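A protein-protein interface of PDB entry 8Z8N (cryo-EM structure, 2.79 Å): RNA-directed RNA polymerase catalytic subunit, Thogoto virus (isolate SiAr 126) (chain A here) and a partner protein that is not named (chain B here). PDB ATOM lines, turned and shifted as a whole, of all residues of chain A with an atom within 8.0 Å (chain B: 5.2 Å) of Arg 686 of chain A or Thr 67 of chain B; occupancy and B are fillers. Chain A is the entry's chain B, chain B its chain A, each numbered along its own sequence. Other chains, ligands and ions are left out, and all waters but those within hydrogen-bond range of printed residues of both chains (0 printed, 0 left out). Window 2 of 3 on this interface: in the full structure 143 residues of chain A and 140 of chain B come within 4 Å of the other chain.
Glu 689 of chain A touches none of the printed residues of chain B. Of the printed residues of chain B, Leu 690 of chain A touches Ser 66 and Trp 70. Val 691 of chain A touches none of the printed residues of chain B. Of the printed residues of chain B, Glu 693 of chain A touches Trp 70. Of the printed residues of chain A, Asp 64 of chain B touches Arg 686. Of the printed residues of chain A, Ser 66 of chain B touches Leu 690 (3.5 Å). Thr 67 of chain B touches just one residue of chain A: Arg 686. The nearest residue of chain B that does not touch Arg 686 of chain A is Gln 63 of chain B (4.8 Å). The nearest printed residue of chain B that does not touch Glu 693 of chain A is Ile 71 of chain B (9.3 Å).
The backbone NH (N) of Ser 66 of chain B lies close to the side-chain carboxylate (OE1) of Glu 69 of chain B (3.4 Å). O of Leu 690 of chain A lies close to NE of Arg 694 of chain A, 3.3 Å away. The side-chain amide nitrogen of Gln 63 of chain B is in hydrogen-bond range of the side-chain hydroxyl of Thr 67 of chain B (2.4 Å). The backbone carbonyl oxygen of Asp 64 of chain B is in hydrogen-bond range of the side-chain hydroxyl of Thr 67 of chain B, 2.6 Å away. The guanidinium group (NH1) of Arg 686 of chain A lies within salt-bridge range of the side-chain carboxylate (OE2) of Glu 689 of chain A, at 2.5 Å.
OD2 of Asp 64 of chain B touches CB of Arg 686 of chain A, at 3.2 Å. NH2 of Arg 686 of chain A touches CG2 of Thr 67 of chain B, at 3.7 Å. CD2 of Leu 690 of chain A touches OG of Ser 66 of chain B, at 3.5 Å. CB of Trp 70 of chain B touches CD1 of Leu 690 of chain A (3.5 Å). Trp 70 of chain B touches Glu 693 of chain A (CH2 to CB, 3.5 Å). Arg 694 of chain A touches Trp 70 of chain B (CG to NE1, 3.4 Å).
Of the 19 printed residues of chain A, 4 touch a printed residue of chain B. Of the 10 printed residues of chain B, 4 touch a printed residue of chain A. Along chain B the printed residues that touch a printed residue of chain A span positions 64 to 70. Among the printed residues, no Asp or Glu carboxylate lies within 4 Å of a Lys or Arg side-chain nitrogen of the other chain.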
ATOM      1  N   LEU A 665     -13.844   6.614   3.056  1.00  0.00           N
ATOM      2  CA  LEU A 665     -12.567   6.566   2.351  1.00  0.00           C
ATOM      3  C   LEU A 665     -12.476   7.633   1.270  1.00  0.00           C
ATOM      4  O   LEU A 665     -11.379   8.116   0.970  1.00  0.00           O
ATOM      5  CB  LEU A 665     -12.349   5.176   1.755  1.00  0.00           C
ATOM      6  CG  LEU A 665     -11.625   4.197   2.680  1.00  0.00           C
ATOM      7  CD1 LEU A 665     -11.797   2.767   2.205  1.00  0.00           C
ATOM      8  CD2 LEU A 665     -10.153   4.559   2.780  1.00  0.00           C
ATOM      9  N   PHE A 666     -13.606   8.014   0.675  1.00  0.00           N
ATOM     10  CA  PHE A 666     -13.634   9.078  -0.323  1.00  0.00           C
ATOM     11  C   PHE A 666     -14.321  10.306   0.255  1.00  0.00           C
ATOM     12  O   PHE A 666     -15.560  10.357   0.308  1.00  0.00           O
ATOM     13  CB  PHE A 666     -14.350   8.617  -1.597  1.00  0.00           C
ATOM     14  CG  PHE A 666     -13.670   7.479  -2.300  1.00  0.00           C
ATOM     15  CD1 PHE A 666     -13.949   6.167  -1.963  1.00  0.00           C
ATOM     16  CD2 PHE A 666     -12.757   7.725  -3.310  1.00  0.00           C
ATOM     17  CE1 PHE A 666     -13.323   5.124  -2.615  1.00  0.00           C
ATOM     18  CE2 PHE A 666     -12.130   6.686  -3.964  1.00  0.00           C
ATOM     19  CZ  PHE A 666     -12.413   5.383  -3.616  1.00  0.00           C
ATOM     20  N   VAL A 680     -15.723  -1.003  -7.451  1.00  0.00           N
ATOM     21  CA  VAL A 680     -15.673  -0.514  -6.076  1.00  0.00           C
ATOM     22  C   VAL A 680     -14.491  -1.124  -5.331  1.00  0.00           C
ATOM     23  O   VAL A 680     -13.802  -0.437  -4.565  1.00  0.00           O
ATOM     24  CB  VAL A 680     -17.007  -0.802  -5.365  1.00  0.00           C
ATOM     25  CG1 VAL A 680     -16.946  -0.371  -3.916  1.00  0.00           C
ATOM     26  CG2 VAL A 680     -18.149  -0.096  -6.077  1.00  0.00           C
ATOM     27  N   ARG A 681     -14.234  -2.417  -5.547  1.00  0.00           N
ATOM     28  CA  ARG A 681     -13.190  -3.113  -4.801  1.00  0.00           C
ATOM     29  C   ARG A 681     -11.819  -2.489  -5.040  1.00  0.00           C
ATOM     30  O   ARG A 681     -11.113  -2.130  -4.089  1.00  0.00           O
ATOM     31  CB  ARG A 681     -13.175  -4.590  -5.193  1.00  0.00           C
ATOM     32  CG  ARG A 681     -12.223  -5.448  -4.381  1.00  0.00           C
ATOM     33  CD  ARG A 681     -12.288  -6.896  -4.831  1.00  0.00           C
ATOM     34  NE  ARG A 681     -13.593  -7.494  -4.576  1.00  0.00           N
ATOM     35  CZ  ARG A 681     -13.956  -8.031  -3.420  1.00  0.00           C
ATOM     36  NH1 ARG A 681     -13.131  -8.068  -2.387  1.00  0.00           N
ATOM     37  NH2 ARG A 681     -15.176  -8.546  -3.298  1.00  0.00           N
ATOM     38  N   GLU A 682     -11.428  -2.348  -6.309  1.00  0.00           N
ATOM     39  CA  GLU A 682     -10.104  -1.818  -6.616  1.00  0.00           C
ATOM     40  C   GLU A 682      -9.976  -0.358  -6.203  1.00  0.00           C
ATOM     41  O   GLU A 682      -8.930   0.053  -5.689  1.00  0.00           O
ATOM     42  CB  GLU A 682      -9.795  -1.987  -8.104  1.00  0.00           C
ATOM     43  CG  GLU A 682      -9.552  -3.427  -8.529  1.00  0.00           C
ATOM     44  CD  GLU A 682     -10.670  -3.988  -9.379  1.00  0.00           C
ATOM     45  OE1 GLU A 682     -11.828  -3.976  -8.919  1.00  0.00           O
ATOM     46  OE2 GLU A 682     -10.390  -4.443 -10.509  1.00  0.00           O
ATOM     47  N   SER A 683     -11.023   0.440  -6.419  1.00  0.00           N
ATOM     48  CA  SER A 683     -10.970   1.845  -6.026  1.00  0.00           C
ATOM     49  C   SER A 683     -10.779   1.982  -4.521  1.00  0.00           C
ATOM     50  O   SER A 683      -9.924   2.747  -4.057  1.00  0.00           O
ATOM     51  CB  SER A 683     -12.239   2.564  -6.480  1.00  0.00           C
ATOM     52  OG  SER A 683     -12.393   2.490  -7.885  1.00  0.00           O
ATOM     53  N   LEU A 684     -11.558   1.228  -3.740  1.00  0.00           N
ATOM     54  CA  LEU A 684     -11.429   1.295  -2.287  1.00  0.00           C
ATOM     55  C   LEU A 684     -10.065   0.799  -1.828  1.00  0.00           C
ATOM     56  O   LEU A 684      -9.457   1.390  -0.930  1.00  0.00           O
ATOM     57  CB  LEU A 684     -12.541   0.491  -1.617  1.00  0.00           C
ATOM     58  CG  LEU A 684     -13.934   1.116  -1.546  1.00  0.00           C
ATOM     59  CD1 LEU A 684     -14.925   0.098  -1.030  1.00  0.00           C
ATOM     60  CD2 LEU A 684     -13.932   2.345  -0.659  1.00  0.00           C
ATOM     61  N   LYS A 685      -9.568  -0.288  -2.427  1.00  0.00           N
ATOM     62  CA  LYS A 685      -8.268  -0.815  -2.024  1.00  0.00           C
ATOM     63  C   LYS A 685      -7.151   0.178  -2.319  1.00  0.00           C
ATOM     64  O   LYS A 685      -6.274   0.409  -1.475  1.00  0.00           O
ATOM     65  CB  LYS A 685      -8.002  -2.148  -2.724  1.00  0.00           C
ATOM     66  CG  LYS A 685      -6.704  -2.818  -2.308  1.00  0.00           C
ATOM     67  CD  LYS A 685      -6.863  -4.327  -2.223  1.00  0.00           C
ATOM     68  CE  LYS A 685      -7.388  -4.906  -3.527  1.00  0.00           C
ATOM     69  NZ  LYS A 685      -6.568  -4.482  -4.696  1.00  0.00           N
ATOM     70  N   ARG A 686      -7.170   0.784  -3.508  1.00  0.00           N
ATOM     71  CA  ARG A 686      -6.134   1.749  -3.854  1.00  0.00           C
ATOM     72  C   ARG A 686      -6.225   2.994  -2.981  1.00  0.00           C
ATOM     73  O   ARG A 686      -5.196   3.556  -2.592  1.00  0.00           O
ATOM     74  CB  ARG A 686      -6.223   2.118  -5.333  1.00  0.00           C
ATOM     75  CG  ARG A 686      -5.976   0.952  -6.276  1.00  0.00           C
ATOM     76  CD  ARG A 686      -4.546   0.451  -6.170  1.00  0.00           C
ATOM     77  NE  ARG A 686      -3.581   1.455  -6.601  1.00  0.00           N
ATOM     78  CZ  ARG A 686      -2.286   1.416  -6.322  1.00  0.00           C
ATOM     79  NH1 ARG A 686      -1.762   0.433  -5.608  1.00  0.00           N
ATOM     80  NH2 ARG A 686      -1.496   2.388  -6.769  1.00  0.00           N
ATOM     81  N   ARG A 687      -7.441   3.436  -2.651  1.00  0.00           N
ATOM     82  CA  ARG A 687      -7.566   4.594  -1.772  1.00  0.00           C
ATOM     83  C   ARG A 687      -7.089   4.270  -0.361  1.00  0.00           C
ATOM     84  O   ARG A 687      -6.477   5.116   0.300  1.00  0.00           O
ATOM     85  CB  ARG A 687      -9.007   5.102  -1.763  1.00  0.00           C
ATOM     86  CG  ARG A 687      -9.253   6.222  -0.767  1.00  0.00           C
ATOM     87  CD  ARG A 687      -8.421   7.448  -1.113  1.00  0.00           C
ATOM     88  NE  ARG A 687      -8.765   8.017  -2.411  1.00  0.00           N
ATOM     89  CZ  ARG A 687      -9.714   8.921  -2.606  1.00  0.00           C
ATOM     90  NH1 ARG A 687     -10.441   9.386  -1.603  1.00  0.00           N
ATOM     91  NH2 ARG A 687      -9.937   9.372  -3.836  1.00  0.00           N
ATOM     92  N   LEU A 688      -7.349   3.049   0.116  1.00  0.00           N
ATOM     93  CA  LEU A 688      -6.820   2.630   1.410  1.00  0.00           C
ATOM     94  C   LEU A 688      -5.298   2.644   1.406  1.00  0.00           C
ATOM     95  O   LEU A 688      -4.664   3.161   2.335  1.00  0.00           O
ATOM     96  CB  LEU A 688      -7.337   1.236   1.761  1.00  0.00           C
ATOM     97  CG  LEU A 688      -8.548   1.144   2.687  1.00  0.00           C
ATOM     98  CD1 LEU A 688      -9.057  -0.283   2.743  1.00  0.00           C
ATOM     99  CD2 LEU A 688      -8.191   1.641   4.077  1.00  0.00           C
ATOM    100  N   GLU A 689      -4.691   2.080   0.358  1.00  0.00           N
ATOM    101  CA  GLU A 689      -3.235   2.083   0.268  1.00  0.00           C
ATOM    102  C   GLU A 689      -2.691   3.505   0.228  1.00  0.00           C
ATOM    103  O   GLU A 689      -1.702   3.820   0.897  1.00  0.00           O
ATOM    104  CB  GLU A 689      -2.779   1.301  -0.963  1.00  0.00           C
ATOM    105  CG  GLU A 689      -3.194  -0.159  -0.965  1.00  0.00           C
ATOM    106  CD  GLU A 689      -2.881  -0.849  -2.276  1.00  0.00           C
ATOM    107  OE1 GLU A 689      -2.956  -2.095  -2.327  1.00  0.00           O
ATOM    108  OE2 GLU A 689      -2.560  -0.146  -3.257  1.00  0.00           O
ATOM    109  N   LEU A 690      -3.337   4.380  -0.544  1.00  0.00           N
ATOM    110  CA  LEU A 690      -2.871   5.757  -0.662  1.00  0.00           C
ATOM    111  C   LEU A 690      -2.978   6.500   0.664  1.00  0.00           C
ATOM    112  O   LEU A 690      -2.059   7.233   1.047  1.00  0.00           O
ATOM    113  CB  LEU A 690      -3.664   6.479  -1.749  1.00  0.00           C
ATOM    114  CG  LEU A 690      -3.435   7.983  -1.855  1.00  0.00           C
ATOM    115  CD1 LEU A 690      -2.210   8.251  -2.694  1.00  0.00           C
ATOM    116  CD2 LEU A 690      -4.650   8.658  -2.455  1.00  0.00           C
ATOM    117  N   VAL A 691      -4.092   6.328   1.379  1.00  0.00           N
ATOM    118  CA  VAL A 691      -4.269   7.047   2.635  1.00  0.00           C
ATOM    119  C   VAL A 691      -3.337   6.500   3.710  1.00  0.00           C
ATOM    120  O   VAL A 691      -2.886   7.250   4.584  1.00  0.00           O
ATOM    121  CB  VAL A 691      -5.746   7.015   3.079  1.00  0.00           C
ATOM    122  CG1 VAL A 691      -6.147   5.640   3.588  1.00  0.00           C
ATOM    123  CG2 VAL A 691      -6.005   8.078   4.138  1.00  0.00           C
ATOM    124  N   VAL A 692      -3.026   5.201   3.674  1.00  0.00           N
ATOM    125  CA  VAL A 692      -2.079   4.656   4.641  1.00  0.00           C
ATOM    126  C   VAL A 692      -0.666   5.146   4.341  1.00  0.00           C
ATOM    127  O   VAL A 692       0.071   5.552   5.248  1.00  0.00           O
ATOM    128  CB  VAL A 692      -2.156   3.120   4.665  1.00  0.00           C
ATOM    129  CG1 VAL A 692      -0.982   2.547   5.439  1.00  0.00           C
ATOM    130  CG2 VAL A 692      -3.468   2.667   5.282  1.00  0.00           C
ATOM    131  N   GLU A 693      -0.267   5.128   3.066  1.00  0.00           N
ATOM    132  CA  GLU A 693       1.088   5.527   2.701  1.00  0.00           C
ATOM    133  C   GLU A 693       1.348   7.012   2.924  1.00  0.00           C
ATOM    134  O   GLU A 693       2.514   7.414   3.005  1.00  0.00           O
ATOM    135  CB  GLU A 693       1.372   5.166   1.242  1.00  0.00           C
ATOM    136  CG  GLU A 693       1.436   3.671   0.970  1.00  0.00           C
ATOM    137  CD  GLU A 693       2.741   3.050   1.428  1.00  0.00           C
ATOM    138  OE1 GLU A 693       3.718   3.799   1.639  1.00  0.00           O
ATOM    139  OE2 GLU A 693       2.790   1.810   1.579  1.00  0.00           O
ATOM    140  N   ARG A 694       0.306   7.832   3.020  1.00  0.00           N
ATOM    141  CA  ARG A 694       0.476   9.254   3.288  1.00  0.00           C
ATOM    142  C   ARG A 694       0.414   9.589   4.772  1.00  0.00           C
ATOM    143  O   ARG A 694       0.552  10.761   5.135  1.00  0.00           O
ATOM    144  CB  ARG A 694      -0.583  10.071   2.542  1.00  0.00           C
ATOM    145  CG  ARG A 694      -0.429  10.071   1.032  1.00  0.00           C
ATOM    146  CD  ARG A 694      -1.468  10.972   0.387  1.00  0.00           C
ATOM    147  NE  ARG A 694      -2.816  10.444   0.552  1.00  0.00           N
ATOM    148  CZ  ARG A 694      -3.752  11.009   1.301  1.00  0.00           C
ATOM    149  NH1 ARG A 694      -3.524  12.132   1.962  1.00  0.00           N
ATOM    150  NH2 ARG A 694      -4.947  10.432   1.390  1.00  0.00           N
ATOM    151  N   LEU A 706      -0.591  -2.619   5.509  1.00  0.00           N
ATOM    152  CA  LEU A 706      -0.867  -3.199   4.198  1.00  0.00           C
ATOM    153  C   LEU A 706      -0.908  -4.723   4.220  1.00  0.00           C
ATOM    154  O   LEU A 706      -1.566  -5.321   3.363  1.00  0.00           O
ATOM    155  CB  LEU A 706       0.168  -2.733   3.169  1.00  0.00           C
ATOM    156  CG  LEU A 706      -0.070  -1.425   2.405  1.00  0.00           C
ATOM    157  CD1 LEU A 706      -0.415  -0.267   3.321  1.00  0.00           C
ATOM    158  CD2 LEU A 706       1.143  -1.087   1.549  1.00  0.00           C
ATOM    159  N   ILE A 709      -4.557  -6.195   4.533  1.00  0.00           N
ATOM    160  CA  ILE A 709      -5.570  -5.788   3.566  1.00  0.00           C
ATOM    161  C   ILE A 709      -5.770  -6.920   2.566  1.00  0.00           C
ATOM    162  O   ILE A 709      -4.827  -7.326   1.879  1.00  0.00           O
ATOM    163  CB  ILE A 709      -5.172  -4.487   2.852  1.00  0.00           C
ATOM    164  CG1 ILE A 709      -5.078  -3.334   3.852  1.00  0.00           C
ATOM    165  CG2 ILE A 709      -6.169  -4.159   1.752  1.00  0.00           C
ATOM    166  CD1 ILE A 709      -4.523  -2.058   3.259  1.00  0.00           C
ATOM    167  N   GLN B  63      -4.509   4.081 -14.251  1.00  0.00           N
ATOM    168  CA  GLN B  63      -4.570   3.818 -12.823  1.00  0.00           C
ATOM    169  C   GLN B  63      -5.250   4.993 -12.134  1.00  0.00           C
ATOM    170  O   GLN B  63      -5.427   6.064 -12.721  1.00  0.00           O
ATOM    171  CB  GLN B  63      -3.173   3.571 -12.234  1.00  0.00           C
ATOM    172  CG  GLN B  63      -2.336   4.822 -12.063  1.00  0.00           C
ATOM    173  CD  GLN B  63      -0.967   4.534 -11.480  1.00  0.00           C
ATOM    174  OE1 GLN B  63      -0.257   3.641 -11.941  1.00  0.00           O
ATOM    175  NE2 GLN B  63      -0.585   5.296 -10.461  1.00  0.00           N
ATOM    176  N   ASP B  64      -5.642   4.776 -10.878  1.00  0.00           N
ATOM    177  CA  ASP B  64      -6.428   5.764 -10.150  1.00  0.00           C
ATOM    178  C   ASP B  64      -5.685   7.091 -10.052  1.00  0.00           C
ATOM    179  O   ASP B  64      -4.503   7.131  -9.702  1.00  0.00           O
ATOM    180  CB  ASP B  64      -6.772   5.239  -8.757  1.00  0.00           C
ATOM    181  CG  ASP B  64      -7.754   4.084  -8.799  1.00  0.00           C
ATOM    182  OD1 ASP B  64      -8.570   4.031  -9.743  1.00  0.00           O
ATOM    183  OD2 ASP B  64      -7.711   3.231  -7.891  1.00  0.00           O
ATOM    184  N   ARG B  65      -6.406   8.180 -10.337  1.00  0.00           N
ATOM    185  CA  ARG B  65      -5.777   9.486 -10.525  1.00  0.00           C
ATOM    186  C   ARG B  65      -5.050   9.950  -9.268  1.00  0.00           C
ATOM    187  O   ARG B  65      -3.923  10.462  -9.345  1.00  0.00           O
ATOM    188  CB  ARG B  65      -6.835  10.504 -10.948  1.00  0.00           C
ATOM    189  CG  ARG B  65      -6.315  11.910 -11.166  1.00  0.00           C
ATOM    190  CD  ARG B  65      -5.370  11.976 -12.351  1.00  0.00           C
ATOM    191  NE  ARG B  65      -6.054  11.692 -13.606  1.00  0.00           N
ATOM    192  CZ  ARG B  65      -5.442  11.467 -14.759  1.00  0.00           C
ATOM    193  NH1 ARG B  65      -4.122  11.485 -14.855  1.00  0.00           N
ATOM    194  NH2 ARG B  65      -6.170  11.216 -15.844  1.00  0.00           N
ATOM    195  N   SER B  66      -5.671   9.762  -8.099  1.00  0.00           N
ATOM    196  CA  SER B  66      -5.083  10.236  -6.851  1.00  0.00           C
ATOM    197  C   SER B  66      -3.675   9.693  -6.651  1.00  0.00           C
ATOM    198  O   SER B  66      -2.823  10.374  -6.070  1.00  0.00           O
ATOM    199  CB  SER B  66      -5.975   9.846  -5.672  1.00  0.00           C
ATOM    200  OG  SER B  66      -6.117   8.439  -5.587  1.00  0.00           O
ATOM    201  N   THR B  67      -3.404   8.483  -7.146  1.00  0.00           N
ATOM    202  CA  THR B  67      -2.040   7.971  -7.122  1.00  0.00           C
ATOM    203  C   THR B  67      -1.114   8.836  -7.971  1.00  0.00           C
ATOM    204  O   THR B  67       0.027   9.105  -7.574  1.00  0.00           O
ATOM    205  CB  THR B  67      -2.010   6.521  -7.601  1.00  0.00           C
ATOM    206  OG1 THR B  67      -2.110   6.484  -9.030  1.00  0.00           O
ATOM    207  CG2 THR B  67      -3.163   5.737  -6.994  1.00  0.00           C
ATOM    208  N   ILE B  68      -1.580   9.278  -9.143  1.00  0.00           N
ATOM    209  CA  ILE B  68      -0.756  10.152  -9.975  1.00  0.00           C
ATOM    210  C   ILE B  68      -0.476  11.467  -9.259  1.00  0.00           C
ATOM    211  O   ILE B  68       0.661  11.951  -9.253  1.00  0.00           O
ATOM    212  CB  ILE B  68      -1.397  10.388 -11.358  1.00  0.00           C
ATOM    213  CG1 ILE B  68      -1.511   9.087 -12.158  1.00  0.00           C
ATOM    214  CG2 ILE B  68      -0.602  11.416 -12.147  1.00  0.00           C
ATOM    215  CD1 ILE B  68      -2.769   8.319 -11.943  1.00  0.00           C
ATOM    216  N   GLU B  69      -1.501  12.071  -8.644  1.00  0.00           N
ATOM    217  CA  GLU B  69      -1.218  13.312  -7.916  1.00  0.00           C
ATOM    218  C   GLU B  69      -0.280  13.083  -6.737  1.00  0.00           C
ATOM    219  O   GLU B  69       0.555  13.945  -6.446  1.00  0.00           O
ATOM    220  CB  GLU B  69      -2.489  14.016  -7.431  1.00  0.00           C
ATOM    221  CG  GLU B  69      -3.221  14.820  -8.500  1.00  0.00           C
ATOM    222  CD  GLU B  69      -4.270  14.029  -9.227  1.00  0.00           C
ATOM    223  OE1 GLU B  69      -4.531  12.890  -8.810  1.00  0.00           O
ATOM    224  OE2 GLU B  69      -4.831  14.547 -10.215  1.00  0.00           O
ATOM    225  N   TRP B  70      -0.392  11.944  -6.050  1.00  0.00           N
ATOM    226  CA  TRP B  70       0.517  11.668  -4.942  1.00  0.00           C
ATOM    227  C   TRP B  70       1.956  11.540  -5.426  1.00  0.00           C
ATOM    228  O   TRP B  70       2.873  12.135  -4.849  1.00  0.00           O
ATOM    229  CB  TRP B  70       0.094  10.397  -4.212  1.00  0.00           C
ATOM    230  CG  TRP B  70       0.948  10.103  -3.019  1.00  0.00           C
ATOM    231  CD1 TRP B  70       1.358  10.989  -2.066  1.00  0.00           C
ATOM    232  CD2 TRP B  70       1.525   8.841  -2.668  1.00  0.00           C
ATOM    233  NE1 TRP B  70       2.141  10.353  -1.135  1.00  0.00           N
ATOM    234  CE2 TRP B  70       2.261   9.034  -1.482  1.00  0.00           C
ATOM    235  CE3 TRP B  70       1.486   7.564  -3.238  1.00  0.00           C
ATOM    236  CZ2 TRP B  70       2.951   7.999  -0.856  1.00  0.00           C
ATOM    237  CZ3 TRP B  70       2.172   6.539  -2.615  1.00  0.00           C
ATOM    238  CH2 TRP B  70       2.895   6.762  -1.438  1.00  0.00           C
ATOM    239  N   ILE B  71       2.173  10.757  -6.485  1.00  0.00           N
ATOM    240  CA  ILE B  71       3.532  10.545  -6.976  1.00  0.00           C
ATOM    241  C   ILE B  71       4.108  11.837  -7.544  1.00  0.00           C
ATOM    242  O   ILE B  71       5.291  12.140  -7.350  1.00  0.00           O
ATOM    243  CB  ILE B  71       3.563   9.403  -8.007  1.00  0.00           C
ATOM    244  CG1 ILE B  71       2.931   8.139  -7.423  1.00  0.00           C
ATOM    245  CG2 ILE B  71       4.989   9.114  -8.438  1.00  0.00           C
ATOM    246  CD1 ILE B  71       2.888   6.976  -8.389  1.00  0.00           C
ATOM    247  N   CYS B  72       3.288  12.621  -8.247  1.00  0.00           N
ATOM    248  CA  CYS B  72       3.770  13.878  -8.808  1.00  0.00           C
ATOM    249  C   CYS B  72       4.061  14.901  -7.716  1.00  0.00           C
ATOM    250  O   CYS B  72       4.986  15.712  -7.850  1.00  0.00           O
ATOM    251  CB  CYS B  72       2.754  14.427  -9.809  1.00  0.00           C
ATOM    252  SG  CYS B  72       2.527  13.409 -11.286  1.00  0.00           S
